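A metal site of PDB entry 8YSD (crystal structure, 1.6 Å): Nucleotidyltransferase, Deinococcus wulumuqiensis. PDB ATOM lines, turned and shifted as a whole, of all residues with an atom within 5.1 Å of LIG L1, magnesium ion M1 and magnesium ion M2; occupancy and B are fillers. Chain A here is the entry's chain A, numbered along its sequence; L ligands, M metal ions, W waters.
O3 of LIG L1 is in salt-bridge range of NZ of Lys 192 (2.7 Å). An oxygen (O1) of LIG L1 is in salt-bridge range of the guanidinium group (NH1) of Arg 195, 2.8 Å away. O5 of LIG L1 lies close to N of Ser 63 (2.8 Å). The side-chain hydroxyl (OG) of Ser 63 sits at hydrogen-bond distance from an oxygen (O3) of LIG L1 (3.1 Å). ND2 of Asn 277 is in hydrogen-bond range of N4 of LIG L1 (3.0 Å).
An oxygen (O7) of LIG L1 lies within hydrogen-bond range of an oxygen (O13) of LG2 L2 (2.6 Å).
The side-chain carboxylate of Asp 79 lies within hydrogen-bond range of a ring nitrogen (NE2) of His 128, at 2.8 Å. N of Gln 61 is in hydrogen-bond range of O of Asp 81, at 3.1 Å. The backbone carbonyl oxygen (O) of Lys 192 lies close to the guanidinium group (NE) of Arg 195, at 3.5 Å. The side-chain amino group (NZ) of Lys 192 is in hydrogen-bond range of the backbone carbonyl oxygen (O) of Thr 68 (2.9 Å). The backbone carbonyl oxygen (O) of Ser 63 sits at hydrogen-bond distance from the backbone NH (N) of Thr 68 (3.0 Å). The backbone carbonyl oxygen (O) of Asn 277 sits at hydrogen-bond distance from the backbone NH (N) of Leu 271 (2.9 Å). OG1 of Thr 213 lies within hydrogen-bond range of O of Gly 209, at 2.8 Å.
Gly 62 touches LIG L1. Met 66 touches LIG L1. CD2 of Phe 168 touches O13 of LIG L1, at 3.7 Å. Gly 209 touches LIG L1. CG2 of Ile 210 touches N2 of LIG L1, at 3.7 Å. Leu 271 touches LIG L1 (CD2 to C9, 3.9 Å). Val 279 touches LIG L1 (CG1 to N4, 3.6 Å). Hydrophobic or aromatic side chains that line LIG L1: Met 66, Phe 168, Ile 210, Leu 271 and Val 279. The nearest printed residue that does not touch LIG L1 is Gln 61 (4.2 Å).
Of the 21 residues printed, 3 come within 4 Å of magnesium ion M1.
Of the 21 residues printed, 2 come within 4 Å of magnesium ion M2. Along chain A the residues within 4 Å of magnesium ion M2 span positions 79 to 81.
Magnesium ion M1 is bound by water W1 (1.9 Å), water W5 (2.1 Å), OD1 of Asp 81 (2.1 Å), OD2 of Asp 130 (2.1 Å), OD2 of Asp 79 (2.3 Å) and O8 of LIG L1 (2.4 Å). Magnesium ion M1 has six donor atoms within binding distance. Slightly farther from magnesium ion M1 lies OD1 of Asp 79 (2.6 Å).
Magnesium ion M2 is bound by an oxygen (O2) of LIG L1. Magnesium ion M2 is bound by OD2 of Asp 79 (2.0 Å). Magnesium ion M2 is bound by O5 of LIG L1 (2.0 Å). Water W10 is bound to magnesium ion M2, 2.0 Å away. Magnesium ion M2 is bound by the side-chain carboxylate (OD2) of Asp 81 (2.1 Å). O8 of LIG L1 is bound to magnesium ion M2, 2.1 Å away.
Water W1 lies within hydrogen-bond range of O12 of LG2 L2 (3.2 Å) and O10 of LIG L1 (3.4 Å). Water W10 bridges the backbone carbonyl oxygen of Asp 79 (2.7 Å) and the side-chain hydroxyl of Ser 63 (2.8 Å). Water W6 lies within hydrogen-bond range of O7 of LIG L1 (2.6 Å), N of Ile 210 (2.9 Å) and O of Ala 206 (3.0 Å). Water W4 bridges O3 of LIG L1 (2.6 Å) and OG of Ser 63 (2.9 Å). Water W8 lies within hydrogen-bond range of an oxygen (O13) of LIG L1 (2.8 Å), the backbone NH of Gly 62 (2.9 Å) and the side-chain amide nitrogen of Gln 61 (3.2 Å). Water W2 lies within hydrogen-bond range of the guanidinium group (NH2) of Arg 195 (2.5 Å) and an oxygen (O3) of LIG L1 (2.9 Å).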
ATOM      1  N   GLN A  61      33.172   6.845  20.171  1.00  0.00           N
ATOM      2  CA  GLN A  61      32.526   5.593  19.792  1.00  0.00           C
ATOM      3  C   GLN A  61      33.096   5.067  18.484  1.00  0.00           C
ATOM      4  O   GLN A  61      33.863   5.754  17.798  1.00  0.00           O
ATOM      5  CB  GLN A  61      31.001   5.747  19.626  1.00  0.00           C
ATOM      6  CG  GLN A  61      30.288   5.925  20.939  1.00  0.00           C
ATOM      7  CD  GLN A  61      28.821   5.591  20.880  1.00  0.00           C
ATOM      8  OE1 GLN A  61      27.991   6.437  21.189  1.00  0.00           O
ATOM      9  NE2 GLN A  61      28.501   4.356  20.567  1.00  0.00           N
ATOM     10  N   GLY A  62      32.677   3.826  18.131  1.00  0.00           N
ATOM     11  CA  GLY A  62      32.906   3.304  16.813  1.00  0.00           C
ATOM     12  C   GLY A  62      34.365   2.951  16.542  1.00  0.00           C
ATOM     13  O   GLY A  62      35.221   2.831  17.446  1.00  0.00           O
ATOM     14  N   SER A  63      34.635   2.785  15.253  1.00  0.00           N
ATOM     15  CA  SER A  63      35.915   2.240  14.858  1.00  0.00           C
ATOM     16  C   SER A  63      37.090   3.160  15.211  1.00  0.00           C
ATOM     17  O   SER A  63      38.196   2.676  15.466  1.00  0.00           O
ATOM     18  CB  SER A  63      35.860   1.945  13.363  1.00  0.00           C
ATOM     19  OG  SER A  63      35.889   3.173  12.653  1.00  0.00           O
ATOM     20  N   MET A  66      37.845   2.233  18.725  1.00  0.00           N
ATOM     21  CA  MET A  66      38.273   0.862  18.898  1.00  0.00           C
ATOM     22  C   MET A  66      39.532   0.547  18.087  1.00  0.00           C
ATOM     23  O   MET A  66      39.977  -0.609  18.076  1.00  0.00           O
ATOM     24  CB  MET A  66      37.143  -0.098  18.501  1.00  0.00           C
ATOM     25  CG  MET A  66      35.871   0.056  19.341  1.00  0.00           C
ATOM     26  SD  MET A  66      34.613  -1.163  19.064  1.00  0.00           S
ATOM     27  CE  MET A  66      33.953  -0.668  17.455  1.00  0.00           C
ATOM     28  N   THR A  68      39.797   0.247  14.837  1.00  0.00           N
ATOM     29  CA  THR A  68      39.467  -0.615  13.710  1.00  0.00           C
ATOM     30  C   THR A  68      39.075   0.188  12.470  1.00  0.00           C
ATOM     31  O   THR A  68      38.393  -0.321  11.561  1.00  0.00           O
ATOM     32  CB  THR A  68      38.317  -1.521  14.090  1.00  0.00           C
ATOM     33  OG1 THR A  68      37.239  -0.693  14.528  1.00  0.00           O
ATOM     34  CG2 THR A  68      38.718  -2.469  15.223  1.00  0.00           C
ATOM     35  N   GLY A  69      39.550   1.420  12.358  1.00  0.00           N
ATOM     36  CA  GLY A  69      39.138   2.298  11.278  1.00  0.00           C
ATOM     37  C   GLY A  69      39.914   2.132   9.984  1.00  0.00           C
ATOM     38  O   GLY A  69      41.114   1.810   9.980  1.00  0.00           O
ATOM     39  N   ASP A  79      33.724   8.367   8.883  1.00  0.00           N
ATOM     40  CA  ASP A  79      32.594   8.216   9.764  1.00  0.00           C
ATOM     41  C   ASP A  79      33.036   8.471  11.203  1.00  0.00           C
ATOM     42  O   ASP A  79      33.542   7.556  11.840  1.00  0.00           O
ATOM     43  CB  ASP A  79      32.084   6.798   9.596  1.00  0.00           C
ATOM     44  CG  ASP A  79      30.964   6.516  10.454  1.00  0.00           C
ATOM     45  OD1 ASP A  79      30.007   7.290  10.335  1.00  0.00           O
ATOM     46  OD2 ASP A  79      31.048   5.595  11.269  1.00  0.00           O
ATOM     47  N   ASP A  81      32.265   8.657  14.871  1.00  0.00           N
ATOM     48  CA  ASP A  81      31.189   8.245  15.767  1.00  0.00           C
ATOM     49  C   ASP A  81      31.461   8.803  17.153  1.00  0.00           C
ATOM     50  O   ASP A  81      32.566   8.635  17.678  1.00  0.00           O
ATOM     51  CB  ASP A  81      31.103   6.719  15.844  1.00  0.00           C
ATOM     52  CG  ASP A  81      30.847   6.084  14.502  1.00  0.00           C
ATOM     53  OD1 ASP A  81      29.837   6.433  13.875  1.00  0.00           O
ATOM     54  OD2 ASP A  81      31.656   5.217  14.075  1.00  0.00           O
ATOM     55  N   HIS A 128      31.237  12.398   7.704  1.00  0.00           N
ATOM     56  CA  HIS A 128      30.069  12.745   8.481  1.00  0.00           C
ATOM     57  C   HIS A 128      30.356  12.391   9.930  1.00  0.00           C
ATOM     58  O   HIS A 128      31.242  11.591  10.235  1.00  0.00           O
ATOM     59  CB  HIS A 128      28.772  12.082   7.999  1.00  0.00           C
ATOM     60  CG  HIS A 128      28.839  10.593   7.893  1.00  0.00           C
ATOM     61  ND1 HIS A 128      29.309   9.945   6.768  1.00  0.00           N
ATOM     62  CD2 HIS A 128      28.471   9.617   8.763  1.00  0.00           C
ATOM     63  CE1 HIS A 128      29.229   8.641   6.951  1.00  0.00           C
ATOM     64  NE2 HIS A 128      28.744   8.417   8.157  1.00  0.00           N
ATOM     65  N   ASP A 130      28.475  11.027  13.309  1.00  0.00           N
ATOM     66  CA  ASP A 130      27.309  10.284  13.809  1.00  0.00           C
ATOM     67  C   ASP A 130      27.284  10.484  15.328  1.00  0.00           C
ATOM     68  O   ASP A 130      28.052   9.870  16.061  1.00  0.00           O
ATOM     69  CB  ASP A 130      27.411   8.794  13.478  1.00  0.00           C
ATOM     70  CG  ASP A 130      27.352   8.498  11.974  1.00  0.00           C
ATOM     71  OD1 ASP A 130      26.813   9.337  11.228  1.00  0.00           O
ATOM     72  OD2 ASP A 130      27.861   7.436  11.551  1.00  0.00           O
ATOM     73  N   PRO A 165      27.742   0.986  24.975  1.00  0.00           N
ATOM     74  CA  PRO A 165      28.857   1.150  24.013  1.00  0.00           C
ATOM     75  C   PRO A 165      30.220   1.011  24.669  1.00  0.00           C
ATOM     76  O   PRO A 165      31.138   0.459  24.039  1.00  0.00           O
ATOM     77  CB  PRO A 165      28.619   2.558  23.442  1.00  0.00           C
ATOM     78  CG  PRO A 165      27.817   3.256  24.497  1.00  0.00           C
ATOM     79  CD  PRO A 165      26.910   2.194  25.030  1.00  0.00           C
ATOM     80  N   PHE A 168      30.940  -2.667  25.037  1.00  0.00           N
ATOM     81  CA  PHE A 168      31.288  -3.250  23.737  1.00  0.00           C
ATOM     82  C   PHE A 168      32.720  -2.888  23.349  1.00  0.00           C
ATOM     83  O   PHE A 168      33.503  -3.748  22.930  1.00  0.00           O
ATOM     84  CB  PHE A 168      30.293  -2.806  22.640  1.00  0.00           C
ATOM     85  CG  PHE A 168      30.618  -3.363  21.292  1.00  0.00           C
ATOM     86  CD1 PHE A 168      30.657  -4.716  21.077  1.00  0.00           C
ATOM     87  CD2 PHE A 168      30.902  -2.517  20.229  1.00  0.00           C
ATOM     88  CE1 PHE A 168      31.002  -5.261  19.828  1.00  0.00           C
ATOM     89  CE2 PHE A 168      31.232  -3.036  18.982  1.00  0.00           C
ATOM     90  CZ  PHE A 168      31.276  -4.398  18.766  1.00  0.00           C
ATOM     91  N   LYS A 192      36.603  -4.687   6.125  1.00  0.00           N
ATOM     92  CA  LYS A 192      35.905  -3.437   5.865  1.00  0.00           C
ATOM     93  C   LYS A 192      36.277  -2.922   4.482  1.00  0.00           C
ATOM     94  O   LYS A 192      35.417  -2.409   3.768  1.00  0.00           O
ATOM     95  CB  LYS A 192      36.255  -2.396   6.949  1.00  0.00           C
ATOM     96  CG  LYS A 192      35.517  -2.697   8.270  1.00  0.00           C
ATOM     97  CD  LYS A 192      35.882  -1.690   9.309  1.00  0.00           C
ATOM     98  CE  LYS A 192      35.077  -1.817  10.606  1.00  0.00           C
ATOM     99  NZ  LYS A 192      35.485  -0.708  11.568  1.00  0.00           N
ATOM    100  N   ARG A 195      34.261  -4.923   2.125  1.00  0.00           N
ATOM    101  CA  ARG A 195      32.934  -4.315   2.127  1.00  0.00           C
ATOM    102  C   ARG A 195      32.885  -3.140   1.171  1.00  0.00           C
ATOM    103  O   ARG A 195      31.963  -3.030   0.334  1.00  0.00           O
ATOM    104  CB  ARG A 195      32.579  -3.852   3.536  1.00  0.00           C
ATOM    105  CG  ARG A 195      31.251  -3.062   3.660  1.00  0.00           C
ATOM    106  CD  ARG A 195      31.264  -2.141   4.924  1.00  0.00           C
ATOM    107  NE  ARG A 195      32.368  -1.199   4.918  1.00  0.00           N
ATOM    108  CZ  ARG A 195      32.782  -0.513   5.989  1.00  0.00           C
ATOM    109  NH1 ARG A 195      32.213  -0.691   7.177  1.00  0.00           N
ATOM    110  NH2 ARG A 195      33.820   0.333   5.886  1.00  0.00           N
ATOM    111  N   ALA A 206      25.514  -1.025   5.124  1.00  0.00           N
ATOM    112  CA  ALA A 206      25.778  -0.257   6.347  1.00  0.00           C
ATOM    113  C   ALA A 206      25.987  -1.129   7.581  1.00  0.00           C
ATOM    114  O   ALA A 206      26.883  -0.799   8.379  1.00  0.00           O
ATOM    115  CB  ALA A 206      24.648   0.749   6.586  1.00  0.00           C
ATOM    116  N   GLY A 209      29.971  -3.093   8.765  1.00  0.00           N
ATOM    117  CA  GLY A 209      31.080  -2.645   9.596  1.00  0.00           C
ATOM    118  C   GLY A 209      31.010  -3.190  11.036  1.00  0.00           C
ATOM    119  O   GLY A 209      31.867  -3.989  11.489  1.00  0.00           O
ATOM    120  N   ILE A 210      29.961  -2.766  11.733  1.00  0.00           N
ATOM    121  CA  ILE A 210      29.708  -3.278  13.075  1.00  0.00           C
ATOM    122  C   ILE A 210      29.457  -4.783  13.048  1.00  0.00           C
ATOM    123  O   ILE A 210      29.936  -5.520  13.924  1.00  0.00           O
ATOM    124  CB  ILE A 210      28.546  -2.510  13.739  1.00  0.00           C
ATOM    125  CG1 ILE A 210      28.278  -3.048  15.130  1.00  0.00           C
ATOM    126  CG2 ILE A 210      27.266  -2.666  12.931  1.00  0.00           C
ATOM    127  CD1 ILE A 210      29.454  -2.975  16.045  1.00  0.00           C
ATOM    128  N   THR A 213      32.667  -6.550  12.847  1.00  0.00           N
ATOM    129  CA  THR A 213      33.418  -6.398  14.093  1.00  0.00           C
ATOM    130  C   THR A 213      32.885  -7.349  15.145  1.00  0.00           C
ATOM    131  O   THR A 213      33.668  -8.041  15.826  1.00  0.00           O
ATOM    132  CB  THR A 213      33.352  -4.950  14.573  1.00  0.00           C
ATOM    133  OG1 THR A 213      33.858  -4.117  13.520  1.00  0.00           O
ATOM    134  CG2 THR A 213      34.174  -4.681  15.869  1.00  0.00           C
ATOM    135  N   LEU A 271      25.104  -8.732  19.427  1.00  0.00           N
ATOM    136  CA  LEU A 271      26.020  -7.863  20.171  1.00  0.00           C
ATOM    137  C   LEU A 271      26.364  -8.563  21.482  1.00  0.00           C
ATOM    138  O   LEU A 271      25.468  -9.100  22.135  1.00  0.00           O
ATOM    139  CB  LEU A 271      25.354  -6.529  20.465  1.00  0.00           C
ATOM    140  CG  LEU A 271      26.288  -5.373  20.796  1.00  0.00           C
ATOM    141  CD1 LEU A 271      27.047  -4.908  19.560  1.00  0.00           C
ATOM    142  CD2 LEU A 271      25.469  -4.199  21.327  1.00  0.00           C
ATOM    143  N   ASN A 277      21.265  -7.216  20.652  1.00  0.00           N
ATOM    144  CA  ASN A 277      20.505  -7.293  19.404  1.00  0.00           C
ATOM    145  C   ASN A 277      21.339  -7.933  18.301  1.00  0.00           C
ATOM    146  O   ASN A 277      22.573  -7.868  18.326  1.00  0.00           O
ATOM    147  CB  ASN A 277      20.080  -5.892  18.972  1.00  0.00           C
ATOM    148  CG  ASN A 277      21.278  -4.983  18.713  1.00  0.00           C
ATOM    149  OD1 ASN A 277      22.052  -4.655  19.638  1.00  0.00           O
ATOM    150  ND2 ASN A 277      21.451  -4.585  17.462  1.00  0.00           N
ATOM    151  N   VAL A 279      23.097  -7.664  15.197  1.00  0.00           N
ATOM    152  CA  VAL A 279      23.521  -6.466  14.501  1.00  0.00           C
ATOM    153  C   VAL A 279      23.284  -6.552  12.998  1.00  0.00           C
ATOM    154  O   VAL A 279      23.391  -5.537  12.310  1.00  0.00           O
ATOM    155  CB  VAL A 279      25.006  -6.185  14.802  1.00  0.00           C
ATOM    156  CG1 VAL A 279      25.176  -5.907  16.312  1.00  0.00           C
ATOM    157  CG2 VAL A 279      25.849  -7.343  14.357  1.00  0.00           C
HETATM  158  P1  LIG L   1      32.771   1.429  10.664  1.00  0.00           P
HETATM  159  O1  LIG L   1      32.106   0.609   9.628  1.00  0.00           O
HETATM  160  O2  LIG L   1      32.088   2.749  10.891  1.00  0.00           O
HETATM  161  O3  LIG L   1      34.263   1.507  10.546  1.00  0.00           O
HETATM  162  P2  LIG L   1      31.931   1.128  13.347  1.00  0.00           P
HETATM  163  O4  LIG L   1      32.187   0.188  14.498  1.00  0.00           O
HETATM  164  O5  LIG L   1      32.362   2.552  13.574  1.00  0.00           O
HETATM  165  O6  LIG L   1      32.503   0.528  11.992  1.00  0.00           O
HETATM  166  P3  LIG L   1      29.190   2.243  12.976  1.00  0.00           P
HETATM  167  O7  LIG L   1      28.116   1.669  12.102  1.00  0.00           O
HETATM  168  O8  LIG L   1      29.825   3.535  12.613  1.00  0.00           O
HETATM  169  O9  LIG L   1      30.325   1.087  13.173  1.00  0.00           O
HETATM  170  O10 LIG L   1      28.544   2.394  14.449  1.00  0.00           O
HETATM  171  C1  LIG L   1      29.215   3.103  15.483  1.00  0.00           C
HETATM  172  C2  LIG L   1      29.056   2.290  16.787  1.00  0.00           C
HETATM  173  O11 LIG L   1      27.655   2.247  17.062  1.00  0.00           O
HETATM  174  C3  LIG L   1      29.430   0.824  16.710  1.00  0.00           C
HETATM  175  O12 LIG L   1      30.828   0.587  16.960  1.00  0.00           O
HETATM  176  C4  LIG L   1      28.585   0.209  17.809  1.00  0.00           C
HETATM  177  O13 LIG L   1      29.144   0.524  19.107  1.00  0.00           O
HETATM  178  C5  LIG L   1      27.297   0.995  17.655  1.00  0.00           C
HETATM  179  N1  LIG L   1      26.389   0.301  16.734  1.00  0.00           N
HETATM  180  C6  LIG L   1      26.207   0.596  15.423  1.00  0.00           C
HETATM  181  N2  LIG L   1      25.273  -0.200  14.870  1.00  0.00           N
HETATM  182  C7  LIG L   1      24.831  -1.020  15.826  1.00  0.00           C
HETATM  183  C8  LIG L   1      23.844  -2.108  15.869  1.00  0.00           C
HETATM  184  N3  LIG L   1      23.115  -2.486  14.794  1.00  0.00           N
HETATM  185  N4  LIG L   1      23.692  -2.674  17.074  1.00  0.00           N
HETATM  186  C9  LIG L   1      24.387  -2.293  18.160  1.00  0.00           C
HETATM  187  N5  LIG L   1      25.306  -1.332  18.184  1.00  0.00           N
HETATM  188  C10 LIG L   1      25.554  -0.673  17.054  1.00  0.00           C
HETATM  189  P1  LG2 L   2      16.501   2.640   9.181  1.00  0.00           P
HETATM  190  O1  LG2 L   2      17.558   2.230   8.183  1.00  0.00           O
HETATM  191  O2  LG2 L   2      16.180   1.559  10.192  1.00  0.00           O
HETATM  192  O3  LG2 L   2      15.280   3.303   8.600  1.00  0.00           O
HETATM  193  P2  LG2 L   2      18.538   4.546   9.671  1.00  0.00           P
HETATM  194  O4  LG2 L   2      18.637   4.708   8.179  1.00  0.00           O
HETATM  195  O5  LG2 L   2      18.673   5.776  10.537  1.00  0.00           O
HETATM  196  O6  LG2 L   2      17.200   3.770  10.094  1.00  0.00           O
HETATM  197  P3  LG2 L   2      19.963   2.992  11.628  1.00  0.00           P
HETATM  198  O7  LG2 L   2      20.664   1.655  11.545  1.00  0.00           O
HETATM  199  O8  LG2 L   2      18.756   3.095  12.524  1.00  0.00           O
HETATM  200  O9  LG2 L   2      19.650   3.466  10.113  1.00  0.00           O
HETATM  201  O10 LG2 L   2      21.012   4.119  12.081  1.00  0.00           O
HETATM  202  C1  LG2 L   2      21.898   4.640  11.093  1.00  0.00           C
HETATM  203  C2  LG2 L   2      23.317   4.777  11.631  1.00  0.00           C
HETATM  204  O11 LG2 L   2      23.268   4.673  13.058  1.00  0.00           O
HETATM  205  C3  LG2 L   2      24.194   3.648  11.097  1.00  0.00           C
HETATM  206  O12 LG2 L   2      25.525   4.132  10.861  1.00  0.00           O
HETATM  207  C4  LG2 L   2      24.275   2.656  12.228  1.00  0.00           C
HETATM  208  O13 LG2 L   2      25.518   1.953  12.242  1.00  0.00           O
HETATM  209  C5  LG2 L   2      24.083   3.557  13.447  1.00  0.00           C
HETATM  210  N1  LG2 L   2      23.528   2.747  14.569  1.00  0.00           N
HETATM  211  C6  LG2 L   2      22.647   1.732  14.494  1.00  0.00           C
HETATM  212  N2  LG2 L   2      22.397   1.213  15.708  1.00  0.00           N
HETATM  213  C7  LG2 L   2      23.136   1.896  16.593  1.00  0.00           C
HETATM  214  C8  LG2 L   2      23.352   1.849  18.030  1.00  0.00           C
HETATM  215  N3  LG2 L   2      22.699   0.952  18.801  1.00  0.00           N
HETATM  216  N4  LG2 L   2      24.239   2.728  18.529  1.00  0.00           N
HETATM  217  C9  LG2 L   2      24.897   3.636  17.787  1.00  0.00           C
HETATM  218  N5  LG2 L   2      24.727   3.742  16.467  1.00  0.00           N
HETATM  219  C10 LG2 L   2      23.899   2.901  15.829  1.00  0.00           C
HETATM  220 MG    MG M   1      28.945   5.668  12.105  1.00  0.00          MG
HETATM  221 MG    MG M   2      31.860   4.089  12.351  1.00  0.00          MG
HETATM  222  O   HOH W   1      27.379   5.262  13.148  1.00  0.00           O
HETATM  223  O   HOH W   2      34.278   1.968   7.688  1.00  0.00           O
HETATM  224  O   HOH W   3      34.460  -1.472  14.037  1.00  0.00           O
HETATM  225  O   HOH W   4      36.288   2.935   9.744  1.00  0.00           O
HETATM  226  O   HOH W   5      28.373   4.959  10.231  1.00  0.00           O
HETATM  227  O   HOH W   6      28.746  -0.367  10.639  1.00  0.00           O
HETATM  228  O   HOH W   7      30.241   3.175   8.902  1.00  0.00           O
HETATM  229  O   HOH W   8      30.935   2.432  19.979  1.00  0.00           O
HETATM  230  O   HOH W   9      26.847  -0.179  20.842  1.00  0.00           O
HETATM  231  O   HOH W  10      33.724   4.905  12.284  1.00  0.00           O
HETATM  232  O   HOH W  11      21.905  -2.011  19.862  1.00  0.00           O
